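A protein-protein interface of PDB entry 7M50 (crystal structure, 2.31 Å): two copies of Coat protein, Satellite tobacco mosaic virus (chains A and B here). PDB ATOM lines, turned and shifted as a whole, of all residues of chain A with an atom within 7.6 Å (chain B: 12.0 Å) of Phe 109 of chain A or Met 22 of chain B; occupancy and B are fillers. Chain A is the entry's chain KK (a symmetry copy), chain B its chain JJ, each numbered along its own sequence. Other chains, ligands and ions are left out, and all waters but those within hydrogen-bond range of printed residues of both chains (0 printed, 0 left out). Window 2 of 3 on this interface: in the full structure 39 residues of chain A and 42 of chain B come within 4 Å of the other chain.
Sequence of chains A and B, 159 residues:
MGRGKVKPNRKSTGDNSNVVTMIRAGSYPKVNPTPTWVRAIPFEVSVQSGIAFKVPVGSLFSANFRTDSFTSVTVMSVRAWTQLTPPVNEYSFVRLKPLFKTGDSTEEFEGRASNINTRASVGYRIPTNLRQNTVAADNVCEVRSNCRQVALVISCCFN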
ATOM      1  N   VAL A  78     -17.711 -23.717 -18.214  1.00  0.00           N
ATOM      2  CA  VAL A  78     -18.483 -24.927 -18.467  1.00  0.00           C
ATOM      3  C   VAL A  78     -17.908 -25.617 -19.694  1.00  0.00           C
ATOM      4  O   VAL A  78     -17.770 -24.996 -20.753  1.00  0.00           O
ATOM      5  CB  VAL A  78     -19.979 -24.621 -18.677  1.00  0.00           C
ATOM      6  CG1 VAL A  78     -20.739 -25.893 -19.028  1.00  0.00           C
ATOM      7  CG2 VAL A  78     -20.572 -23.967 -17.438  1.00  0.00           C
ATOM      8  N   ALA A  80     -18.195 -29.397 -22.029  1.00  0.00           N
ATOM      9  CA  ALA A  80     -19.124 -30.476 -22.324  1.00  0.00           C
ATOM     10  C   ALA A  80     -18.482 -31.501 -23.247  1.00  0.00           C
ATOM     11  O   ALA A  80     -17.685 -31.159 -24.126  1.00  0.00           O
ATOM     12  CB  ALA A  80     -20.413 -29.944 -22.965  1.00  0.00           C
ATOM     13  N   VAL A  94     -22.097 -31.102 -30.044  1.00  0.00           N
ATOM     14  CA  VAL A  94     -22.645 -30.624 -28.780  1.00  0.00           C
ATOM     15  C   VAL A  94     -22.628 -29.101 -28.797  1.00  0.00           C
ATOM     16  O   VAL A  94     -21.656 -28.483 -29.240  1.00  0.00           O
ATOM     17  CB  VAL A  94     -21.864 -31.192 -27.572  1.00  0.00           C
ATOM     18  CG1 VAL A  94     -20.382 -30.857 -27.678  1.00  0.00           C
ATOM     19  CG2 VAL A  94     -22.446 -30.676 -26.264  1.00  0.00           C
ATOM     20  N   ARG A  95     -23.719 -28.500 -28.328  1.00  0.00           N
ATOM     21  CA  ARG A  95     -23.865 -27.054 -28.288  1.00  0.00           C
ATOM     22  C   ARG A  95     -24.106 -26.594 -26.857  1.00  0.00           C
ATOM     23  O   ARG A  95     -24.655 -27.332 -26.033  1.00  0.00           O
ATOM     24  CB  ARG A  95     -25.018 -26.583 -29.183  1.00  0.00           C
ATOM     25  CG  ARG A  95     -24.942 -27.067 -30.623  1.00  0.00           C
ATOM     26  CD  ARG A  95     -25.924 -26.306 -31.502  1.00  0.00           C
ATOM     27  NE  ARG A  95     -25.997 -26.849 -32.854  1.00  0.00           N
ATOM     28  CZ  ARG A  95     -26.999 -27.585 -33.313  1.00  0.00           C
ATOM     29  NH1 ARG A  95     -28.046 -27.876 -32.558  1.00  0.00           N
ATOM     30  NH2 ARG A  95     -26.951 -28.040 -34.562  1.00  0.00           N
ATOM     31  N   LEU A  96     -23.694 -25.361 -26.570  1.00  0.00           N
ATOM     32  CA  LEU A  96     -23.849 -24.775 -25.244  1.00  0.00           C
ATOM     33  C   LEU A  96     -24.343 -23.344 -25.386  1.00  0.00           C
ATOM     34  O   LEU A  96     -23.747 -22.551 -26.121  1.00  0.00           O
ATOM     35  CB  LEU A  96     -22.527 -24.801 -24.465  1.00  0.00           C
ATOM     36  CG  LEU A  96     -21.965 -26.175 -24.095  1.00  0.00           C
ATOM     37  CD1 LEU A  96     -20.630 -26.035 -23.383  1.00  0.00           C
ATOM     38  CD2 LEU A  96     -22.955 -26.938 -23.233  1.00  0.00           C
ATOM     39  N   LYS A  97     -25.428 -23.018 -24.687  1.00  0.00           N
ATOM     40  CA  LYS A  97     -25.984 -21.665 -24.681  1.00  0.00           C
ATOM     41  C   LYS A  97     -26.006 -21.136 -23.255  1.00  0.00           C
ATOM     42  O   LYS A  97     -26.884 -21.520 -22.463  1.00  0.00           O
ATOM     43  CB  LYS A  97     -27.388 -21.641 -25.280  1.00  0.00           C
ATOM     44  CG  LYS A  97     -27.963 -20.239 -25.417  1.00  0.00           C
ATOM     45  CD  LYS A  97     -29.352 -20.251 -26.027  1.00  0.00           C
ATOM     46  CE  LYS A  97     -30.367 -20.824 -25.059  1.00  0.00           C
ATOM     47  NZ  LYS A  97     -31.749 -20.793 -25.614  1.00  0.00           N
ATOM     48  N   PRO A  98     -25.079 -20.253 -22.884  1.00  0.00           N
ATOM     49  CA  PRO A  98     -25.010 -19.795 -21.489  1.00  0.00           C
ATOM     50  C   PRO A  98     -26.268 -19.051 -21.068  1.00  0.00           C
ATOM     51  O   PRO A  98     -26.797 -18.214 -21.803  1.00  0.00           O
ATOM     52  CB  PRO A  98     -23.785 -18.873 -21.479  1.00  0.00           C
ATOM     53  CG  PRO A  98     -22.986 -19.274 -22.679  1.00  0.00           C
ATOM     54  CD  PRO A  98     -23.990 -19.698 -23.704  1.00  0.00           C
ATOM     55  N   SER A 105     -28.182 -15.518 -22.654  1.00  0.00           N
ATOM     56  CA  SER A 105     -27.481 -15.238 -23.896  1.00  0.00           C
ATOM     57  C   SER A 105     -28.001 -16.138 -25.015  1.00  0.00           C
ATOM     58  O   SER A 105     -28.724 -17.109 -24.785  1.00  0.00           O
ATOM     59  CB  SER A 105     -25.975 -15.423 -23.714  1.00  0.00           C
ATOM     60  OG  SER A 105     -25.658 -16.776 -23.434  1.00  0.00           O
ATOM     61  N   THR A 106     -27.617 -15.802 -26.247  1.00  0.00           N
ATOM     62  CA  THR A 106     -28.035 -16.552 -27.425  1.00  0.00           C
ATOM     63  C   THR A 106     -26.867 -17.201 -28.157  1.00  0.00           C
ATOM     64  O   THR A 106     -27.035 -17.644 -29.299  1.00  0.00           O
ATOM     65  CB  THR A 106     -28.815 -15.651 -28.387  1.00  0.00           C
ATOM     66  OG1 THR A 106     -28.098 -14.426 -28.587  1.00  0.00           O
ATOM     67  CG2 THR A 106     -30.198 -15.345 -27.832  1.00  0.00           C
ATOM     68  N   GLU A 107     -25.693 -17.268 -27.536  1.00  0.00           N
ATOM     69  CA  GLU A 107     -24.566 -17.958 -28.145  1.00  0.00           C
ATOM     70  C   GLU A 107     -24.820 -19.460 -28.181  1.00  0.00           C
ATOM     71  O   GLU A 107     -25.482 -20.023 -27.307  1.00  0.00           O
ATOM     72  CB  GLU A 107     -23.274 -17.667 -27.378  1.00  0.00           C
ATOM     73  CG  GLU A 107     -22.652 -16.311 -27.684  1.00  0.00           C
ATOM     74  CD  GLU A 107     -23.497 -15.152 -27.198  1.00  0.00           C
ATOM     75  OE1 GLU A 107     -23.672 -15.012 -25.968  1.00  0.00           O
ATOM     76  OE2 GLU A 107     -23.992 -14.380 -28.046  1.00  0.00           O
ATOM     77  N   GLU A 108     -24.285 -20.111 -29.213  1.00  0.00           N
ATOM     78  CA  GLU A 108     -24.397 -21.558 -29.380  1.00  0.00           C
ATOM     79  C   GLU A 108     -23.008 -22.113 -29.703  1.00  0.00           C
ATOM     80  O   GLU A 108     -22.735 -22.542 -30.827  1.00  0.00           O
ATOM     81  CB  GLU A 108     -25.418 -21.917 -30.461  1.00  0.00           C
ATOM     82  CG  GLU A 108     -26.873 -21.714 -30.050  1.00  0.00           C
ATOM     83  CD  GLU A 108     -27.377 -22.796 -29.110  1.00  0.00           C
ATOM     84  OE1 GLU A 108     -26.613 -23.735 -28.811  1.00  0.00           O
ATOM     85  OE2 GLU A 108     -28.544 -22.708 -28.673  1.00  0.00           O
ATOM     86  N   PHE A 109     -22.127 -22.092 -28.703  1.00  0.00           N
ATOM     87  CA  PHE A 109     -20.787 -22.646 -28.850  1.00  0.00           C
ATOM     88  C   PHE A 109     -20.873 -24.123 -29.201  1.00  0.00           C
ATOM     89  O   PHE A 109     -21.328 -24.935 -28.389  1.00  0.00           O
ATOM     90  CB  PHE A 109     -19.977 -22.442 -27.567  1.00  0.00           C
ATOM     91  CG  PHE A 109     -19.915 -21.014 -27.114  1.00  0.00           C
ATOM     92  CD1 PHE A 109     -19.163 -20.086 -27.812  1.00  0.00           C
ATOM     93  CD2 PHE A 109     -20.606 -20.598 -25.988  1.00  0.00           C
ATOM     94  CE1 PHE A 109     -19.101 -18.769 -27.400  1.00  0.00           C
ATOM     95  CE2 PHE A 109     -20.548 -19.281 -25.570  1.00  0.00           C
ATOM     96  CZ  PHE A 109     -19.795 -18.366 -26.277  1.00  0.00           C
ATOM     97  N   GLU A 110     -20.446 -24.481 -30.408  1.00  0.00           N
ATOM     98  CA  GLU A 110     -20.598 -25.834 -30.923  1.00  0.00           C
ATOM     99  C   GLU A 110     -19.238 -26.447 -31.227  1.00  0.00           C
ATOM    100  O   GLU A 110     -18.361 -25.792 -31.799  1.00  0.00           O
ATOM    101  CB  GLU A 110     -21.470 -25.841 -32.182  1.00  0.00           C
ATOM    102  CG  GLU A 110     -21.733 -27.225 -32.751  1.00  0.00           C
ATOM    103  CD  GLU A 110     -22.731 -27.206 -33.890  1.00  0.00           C
ATOM    104  OE1 GLU A 110     -23.236 -26.113 -34.217  1.00  0.00           O
ATOM    105  OE2 GLU A 110     -23.010 -28.284 -34.458  1.00  0.00           O
ATOM    106  N   GLY A 111     -19.074 -27.708 -30.837  1.00  0.00           N
ATOM    107  CA  GLY A 111     -17.903 -28.488 -31.182  1.00  0.00           C
ATOM    108  C   GLY A 111     -18.292 -29.814 -31.802  1.00  0.00           C
ATOM    109  O   GLY A 111     -19.165 -30.512 -31.281  1.00  0.00           O
ATOM    110  N   SER A 121     -16.544 -32.068 -28.251  1.00  0.00           N
ATOM    111  CA  SER A 121     -16.236 -31.268 -27.076  1.00  0.00           C
ATOM    112  C   SER A 121     -16.321 -29.787 -27.409  1.00  0.00           C
ATOM    113  O   SER A 121     -16.013 -29.364 -28.526  1.00  0.00           O
ATOM    114  CB  SER A 121     -14.841 -31.594 -26.525  1.00  0.00           C
ATOM    115  OG  SER A 121     -13.835 -31.314 -27.483  1.00  0.00           O
ATOM    116  N   VAL A 122     -16.744 -29.006 -26.417  1.00  0.00           N
ATOM    117  CA  VAL A 122     -16.789 -27.553 -26.533  1.00  0.00           C
ATOM    118  C   VAL A 122     -16.951 -26.985 -25.133  1.00  0.00           C
ATOM    119  O   VAL A 122     -17.325 -27.706 -24.201  1.00  0.00           O
ATOM    120  CB  VAL A 122     -17.945 -27.114 -27.474  1.00  0.00           C
ATOM    121  CG1 VAL A 122     -19.283 -27.210 -26.758  1.00  0.00           C
ATOM    122  CG2 VAL A 122     -17.700 -25.710 -28.010  1.00  0.00           C
ATOM    123  N   GLY A 123     -16.662 -25.696 -24.978  1.00  0.00           N
ATOM    124  CA  GLY A 123     -16.800 -25.046 -23.689  1.00  0.00           C
ATOM    125  C   GLY A 123     -16.773 -23.542 -23.838  1.00  0.00           C
ATOM    126  O   GLY A 123     -16.406 -23.004 -24.884  1.00  0.00           O
ATOM    127  N   TYR A 124     -17.177 -22.862 -22.766  1.00  0.00           N
ATOM    128  CA  TYR A 124     -17.167 -21.408 -22.738  1.00  0.00           C
ATOM    129  C   TYR A 124     -16.711 -20.929 -21.369  1.00  0.00           C
ATOM    130  O   TYR A 124     -16.831 -21.636 -20.366  1.00  0.00           O
ATOM    131  CB  TYR A 124     -18.543 -20.817 -23.085  1.00  0.00           C
ATOM    132  CG  TYR A 124     -19.622 -21.061 -22.052  1.00  0.00           C
ATOM    133  CD1 TYR A 124     -19.843 -20.155 -21.020  1.00  0.00           C
ATOM    134  CD2 TYR A 124     -20.436 -22.183 -22.119  1.00  0.00           C
ATOM    135  CE1 TYR A 124     -20.830 -20.368 -20.078  1.00  0.00           C
ATOM    136  CE2 TYR A 124     -21.429 -22.405 -21.182  1.00  0.00           C
ATOM    137  CZ  TYR A 124     -21.621 -21.494 -20.164  1.00  0.00           C
ATOM    138  OH  TYR A 124     -22.606 -21.707 -19.229  1.00  0.00           O
ATOM    139  N   ARG A 125     -16.184 -19.708 -21.343  1.00  0.00           N
ATOM    140  CA  ARG A 125     -15.712 -19.074 -20.123  1.00  0.00           C
ATOM    141  C   ARG A 125     -16.627 -17.914 -19.757  1.00  0.00           C
ATOM    142  O   ARG A 125     -17.007 -17.115 -20.619  1.00  0.00           O
ATOM    143  CB  ARG A 125     -14.277 -18.567 -20.282  1.00  0.00           C
ATOM    144  CG  ARG A 125     -13.758 -17.825 -19.063  1.00  0.00           C
ATOM    145  CD  ARG A 125     -12.393 -17.209 -19.302  1.00  0.00           C
ATOM    146  NE  ARG A 125     -11.964 -16.419 -18.155  1.00  0.00           N
ATOM    147  CZ  ARG A 125     -12.255 -15.137 -17.978  1.00  0.00           C
ATOM    148  NH1 ARG A 125     -12.954 -14.456 -18.871  1.00  0.00           N
ATOM    149  NH2 ARG A 125     -11.833 -14.523 -16.876  1.00  0.00           N
ATOM    150  N   GLU A 142     -28.044 -24.233 -21.690  1.00  0.00           N
ATOM    151  CA  GLU A 142     -28.764 -25.244 -22.449  1.00  0.00           C
ATOM    152  C   GLU A 142     -27.777 -26.100 -23.233  1.00  0.00           C
ATOM    153  O   GLU A 142     -26.717 -25.631 -23.655  1.00  0.00           O
ATOM    154  CB  GLU A 142     -29.775 -24.602 -23.403  1.00  0.00           C
ATOM    155  CG  GLU A 142     -30.973 -23.965 -22.712  1.00  0.00           C
ATOM    156  CD  GLU A 142     -32.018 -23.469 -23.694  1.00  0.00           C
ATOM    157  OE1 GLU A 142     -31.824 -23.652 -24.915  1.00  0.00           O
ATOM    158  OE2 GLU A 142     -33.033 -22.894 -23.248  1.00  0.00           O
ATOM    159  N   ARG A 144     -27.474 -29.035 -26.396  1.00  0.00           N
ATOM    160  CA  ARG A 144     -28.046 -29.705 -27.554  1.00  0.00           C
ATOM    161  C   ARG A 144     -27.009 -30.654 -28.133  1.00  0.00           C
ATOM    162  O   ARG A 144     -25.814 -30.347 -28.144  1.00  0.00           O
ATOM    163  CB  ARG A 144     -28.494 -28.701 -28.624  1.00  0.00           C
ATOM    164  CG  ARG A 144     -29.607 -27.767 -28.181  1.00  0.00           C
ATOM    165  CD  ARG A 144     -29.960 -26.784 -29.285  1.00  0.00           C
ATOM    166  NE  ARG A 144     -31.147 -26.002 -28.961  1.00  0.00           N
ATOM    167  CZ  ARG A 144     -32.389 -26.382 -29.228  1.00  0.00           C
ATOM    168  NH1 ARG A 144     -32.647 -27.534 -29.823  1.00  0.00           N
ATOM    169  NH2 ARG A 144     -33.398 -25.585 -28.887  1.00  0.00           N
ATOM    170  N   THR B  13      -5.766 -19.426 -20.324  1.00  0.00           N
ATOM    171  CA  THR B  13      -5.499 -18.603 -21.498  1.00  0.00           C
ATOM    172  C   THR B  13      -6.591 -17.558 -21.690  1.00  0.00           C
ATOM    173  O   THR B  13      -6.592 -16.824 -22.679  1.00  0.00           O
ATOM    174  CB  THR B  13      -5.395 -19.457 -22.776  1.00  0.00           C
ATOM    175  OG1 THR B  13      -6.694 -19.938 -23.140  1.00  0.00           O
ATOM    176  CG2 THR B  13      -4.469 -20.643 -22.553  1.00  0.00           C
ATOM    177  N   GLY B  14      -7.519 -17.492 -20.739  1.00  0.00           N
ATOM    178  CA  GLY B  14      -8.641 -16.583 -20.852  1.00  0.00           C
ATOM    179  C   GLY B  14      -8.918 -15.770 -19.605  1.00  0.00           C
ATOM    180  O   GLY B  14      -9.134 -16.324 -18.523  1.00  0.00           O
ATOM    181  N   ASP B  15      -8.913 -14.449 -19.750  1.00  0.00           N
ATOM    182  CA  ASP B  15      -9.265 -13.539 -18.669  1.00  0.00           C
ATOM    183  C   ASP B  15      -9.766 -12.240 -19.291  1.00  0.00           C
ATOM    184  O   ASP B  15     -10.025 -12.172 -20.497  1.00  0.00           O
ATOM    185  CB  ASP B  15      -8.077 -13.320 -17.723  1.00  0.00           C
ATOM    186  CG  ASP B  15      -6.843 -12.799 -18.439  1.00  0.00           C
ATOM    187  OD1 ASP B  15      -6.857 -12.714 -19.684  1.00  0.00           O
ATOM    188  OD2 ASP B  15      -5.854 -12.471 -17.750  1.00  0.00           O
ATOM    189  N   ASN B  16      -9.899 -11.210 -18.463  1.00  0.00           N
ATOM    190  CA  ASN B  16     -10.365  -9.879 -18.892  1.00  0.00           C
ATOM    191  C   ASN B  16     -11.757 -10.058 -19.507  1.00  0.00           C
ATOM    192  O   ASN B  16     -12.566 -10.830 -18.967  1.00  0.00           O
ATOM    193  CB  ASN B  16      -9.330  -9.247 -19.804  1.00  0.00           C
ATOM    194  CG  ASN B  16      -9.445  -7.737 -19.862  1.00  0.00           C
ATOM    195  OD1 ASN B  16     -10.471  -7.166 -19.489  1.00  0.00           O
ATOM    196  ND2 ASN B  16      -8.393  -7.082 -20.337  1.00  0.00           N
ATOM    197  N   SER B  17     -12.067  -9.361 -20.604  1.00  0.00           N
ATOM    198  CA  SER B  17     -13.305  -9.538 -21.359  1.00  0.00           C
ATOM    199  C   SER B  17     -14.546  -9.141 -20.566  1.00  0.00           C
ATOM    200  O   SER B  17     -14.492  -8.964 -19.345  1.00  0.00           O
ATOM    201  CB  SER B  17     -13.438 -10.987 -21.840  1.00  0.00           C
ATOM    202  OG  SER B  17     -14.608 -11.161 -22.621  1.00  0.00           O
ATOM    203  N   ASN B  18     -15.674  -8.993 -21.265  1.00  0.00           N
ATOM    204  CA  ASN B  18     -16.949  -8.695 -20.634  1.00  0.00           C
ATOM    205  C   ASN B  18     -18.067  -9.628 -21.075  1.00  0.00           C
ATOM    206  O   ASN B  18     -19.185  -9.509 -20.564  1.00  0.00           O
ATOM    207  CB  ASN B  18     -17.369  -7.244 -20.917  1.00  0.00           C
ATOM    208  CG  ASN B  18     -16.434  -6.234 -20.285  1.00  0.00           C
ATOM    209  OD1 ASN B  18     -16.460  -6.022 -19.073  1.00  0.00           O
ATOM    210  ND2 ASN B  18     -15.608  -5.598 -21.106  1.00  0.00           N
ATOM    211  N   VAL B  19     -17.802 -10.545 -22.005  1.00  0.00           N
ATOM    212  CA  VAL B  19     -18.801 -11.478 -22.502  1.00  0.00           C
ATOM    213  C   VAL B  19     -18.226 -12.888 -22.459  1.00  0.00           C
ATOM    214  O   VAL B  19     -17.036 -13.096 -22.219  1.00  0.00           O
ATOM    215  CB  VAL B  19     -19.268 -11.133 -23.930  1.00  0.00           C
ATOM    216  CG1 VAL B  19     -20.163  -9.910 -23.911  1.00  0.00           C
ATOM    217  CG2 VAL B  19     -18.070 -10.910 -24.840  1.00  0.00           C
ATOM    218  N   VAL B  20     -19.100 -13.864 -22.701  1.00  0.00           N
ATOM    219  CA  VAL B  20     -18.676 -15.256 -22.752  1.00  0.00           C
ATOM    220  C   VAL B  20     -17.750 -15.467 -23.942  1.00  0.00           C
ATOM    221  O   VAL B  20     -17.927 -14.869 -25.013  1.00  0.00           O
ATOM    222  CB  VAL B  20     -19.898 -16.188 -22.820  1.00  0.00           C
ATOM    223  CG1 VAL B  20     -20.671 -16.144 -21.510  1.00  0.00           C
ATOM    224  CG2 VAL B  20     -20.799 -15.804 -23.984  1.00  0.00           C
ATOM    225  N   THR B  21     -16.743 -16.317 -23.755  1.00  0.00           N
ATOM    226  CA  THR B  21     -15.768 -16.630 -24.790  1.00  0.00           C
ATOM    227  C   THR B  21     -15.676 -18.141 -24.948  1.00  0.00           C
ATOM    228  O   THR B  21     -15.741 -18.880 -23.961  1.00  0.00           O
ATOM    229  CB  THR B  21     -14.387 -16.056 -24.453  1.00  0.00           C
ATOM    230  OG1 THR B  21     -13.896 -16.658 -23.250  1.00  0.00           O
ATOM    231  CG2 THR B  21     -14.469 -14.550 -24.259  1.00  0.00           C
ATOM    232  N   MET B  22     -15.515 -18.592 -26.190  1.00  0.00           N
ATOM    233  CA  MET B  22     -15.497 -20.019 -26.484  1.00  0.00           C
ATOM    234  C   MET B  22     -14.184 -20.647 -26.037  1.00  0.00           C
ATOM    235  O   MET B  22     -13.102 -20.127 -26.328  1.00  0.00           O
ATOM    236  CB  MET B  22     -15.711 -20.261 -27.978  1.00  0.00           C
ATOM    237  CG  MET B  22     -15.664 -21.734 -28.372  1.00  0.00           C
ATOM    238  SD  MET B  22     -16.601 -22.108 -29.868  1.00  0.00           S
ATOM    239  CE  MET B  22     -15.839 -20.989 -31.039  1.00  0.00           C
ATOM    240  N   ILE B  23     -14.283 -21.771 -25.332  1.00  0.00           N
ATOM    241  CA  ILE B  23     -13.129 -22.560 -24.923  1.00  0.00           C
ATOM    242  C   ILE B  23     -12.977 -23.722 -25.893  1.00  0.00           C
ATOM    243  O   ILE B  23     -13.934 -24.470 -26.131  1.00  0.00           O
ATOM    244  CB  ILE B  23     -13.280 -23.066 -23.478  1.00  0.00           C
ATOM    245  CG1 ILE B  23     -13.287 -21.895 -22.495  1.00  0.00           C
ATOM    246  CG2 ILE B  23     -12.172 -24.053 -23.139  1.00  0.00           C
ATOM    247  CD1 ILE B  23     -13.454 -22.315 -21.050  1.00  0.00           C
ATOM    248  N   ARG B  24     -11.780 -23.875 -26.456  1.00  0.00           N
ATOM    249  CA  ARG B  24     -11.498 -24.969 -27.386  1.00  0.00           C
ATOM    250  C   ARG B  24     -10.994 -26.183 -26.606  1.00  0.00           C
ATOM    251  O   ARG B  24      -9.813 -26.538 -26.615  1.00  0.00           O
ATOM    252  CB  ARG B  24     -10.504 -24.520 -28.449  1.00  0.00           C
ATOM    253  CG  ARG B  24     -11.085 -23.522 -29.438  1.00  0.00           C
ATOM    254  CD  ARG B  24     -10.022 -22.943 -30.352  1.00  0.00           C
ATOM    255  NE  ARG B  24     -10.609 -22.106 -31.393  1.00  0.00           N
ATOM    256  CZ  ARG B  24     -10.983 -20.846 -31.218  1.00  0.00           C
ATOM    257  NH1 ARG B  24     -10.849 -20.239 -30.050  1.00  0.00           N
ATOM    258  NH2 ARG B  24     -11.510 -20.178 -32.241  1.00  0.00           N
ATOM    259  N   ALA B  25     -11.935 -26.823 -25.916  1.00  0.00           N
ATOM    260  CA  ALA B  25     -11.618 -27.988 -25.105  1.00  0.00           C
ATOM    261  C   ALA B  25     -11.222 -29.170 -25.984  1.00  0.00           C
ATOM    262  O   ALA B  25     -11.518 -29.220 -27.182  1.00  0.00           O
ATOM    263  CB  ALA B  25     -12.807 -28.365 -24.221  1.00  0.00           C
ATOM    264  N   GLY B  26     -10.542 -30.133 -25.367  1.00  0.00           N
ATOM    265  CA  GLY B  26     -10.090 -31.312 -26.079  1.00  0.00           C
ATOM    266  C   GLY B  26     -10.661 -32.601 -25.528  1.00  0.00           C
ATOM    267  O   GLY B  26     -11.866 -32.699 -25.279  1.00  0.00           O
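The backbone carbonyl oxygen (O) of Val 78 of chain A is in hydrogen-bond range of the backbone NH (N) of Tyr 124 of chain A, at 3.0 Å. The backbone NH of Leu 96 of chain A lies within hydrogen-bond range of the backbone carbonyl oxygen of Phe 109 of chain A, at 3.0 Å.
No position is printed for both chains. Of the 15 pairs that touch across the chains among the printed residues, none has its exchanged pair printed and touching as well.
Printed residues of chain A that touch a printed residue of chain B: Glu 107, Phe 109, Ser 121, Gly 123, Tyr 124 and Arg 125. Of the 14 printed residues of chain B, 9 touch a printed residue of chain A. Hydrophobic or aromatic side chains of chain B within 4 Å of the printed part of chain A: Val 20, Met 22 and Ile 23. Among the printed residues, 15 pairs touch across the chains. Among the printed residues, no Asp or Glu carboxylate lies within 4 Å of a Lys or Arg side-chain nitrogen of the other chain.
Among the printed residues, merely in contact across the chains: Tyr 124 of chain A with Thr 21 of chain B (3.1 Å), Arg 125 of chain A with Asp 15 of chain B (3.3 Å), Arg 125 of chain A with Val 20 of chain B (3.3 Å), Gly 123 of chain A with Met 22 of chain B (3.4 Å), Phe 109 of chain A with Met 22 of chain B (3.5 Å), Tyr 124 of chain A with Ile 23 of chain B (3.5 Å), Glu 107 of chain A with Val 20 of chain B (3.6 Å), Phe 109 of chain A with Val 20 of chain B (3.6 Å), Arg 125 of chain A with Asn 16 of chain B (3.6 Å) and Arg 125 of chain A with Ile 23 of chain B (3.8 Å).
The guanidinium group of Arg 125 of chain A sits at hydrogen-bond distance from the backbone carbonyl oxygen of Gly 14 of chain B (2.9 Å). OG of Ser 121 of chain A sits at hydrogen-bond distance from O of Gly 26 of chain B, 3.3 Å away. O of Thr 21 of chain B lies within hydrogen-bond range of N of Arg 125 of chain A, 2.8 Å away. The backbone carbonyl oxygen (O) of Gly 123 of chain A sits at hydrogen-bond distance from the backbone NH (N) of Ile 23 of chain B (2.5 Å). The backbone carbonyl oxygen (O) of Ala 25 of chain B lies within hydrogen-bond range of the side-chain hydroxyl (OG) of Ser 121 of chain A (3.1 Å).
No residue of chain B comes within 4 Å of Val 94 of chain A. No residue of chain B comes within 4 Å of Leu 96 of chain A. No residue of chain B comes within 4 Å of Pro 98 of chain A. Glu 107 of chain A touches just one residue of chain B: Val 20 (3.6 Å). No residue of chain B comes within 4 Å of Glu 108 of chain A. Of the printed residues of chain B, Phe 109 of chain A touches Val 20 (3.6 Å) and Met 22 (3.5 Å). No residue of chain B comes within 4 Å of Gly 111 of chain A. Of chain B, only Thr 21 (3.1 Å) and Ile 23 (3.5 Å) come within 4 Å of Tyr 124 of chain A. Of the printed residues of chain B, Arg 125 of chain A touches Gly 14, Asp 15, Asn 16, Val 20, Thr 21 and Ile 23. Printed residues of chain A within 4 Å of Met 22 of chain B: Phe 109 and Gly 123. Printed residues of chain A within 4 Å of Gly 26 of chain B: Ser 121. The nearest printed residue of chain B that does not touch Phe 109 of chain A is Thr 21 of chain B (4.3 Å). The nearest printed residue of chain A that does not touch Met 22 of chain B is Val 122 of chain A (4.2 Å). The nearest printed residue of chain A that does not touch Ile 23 of chain B is Val 122 of chain A (4.1 Å).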
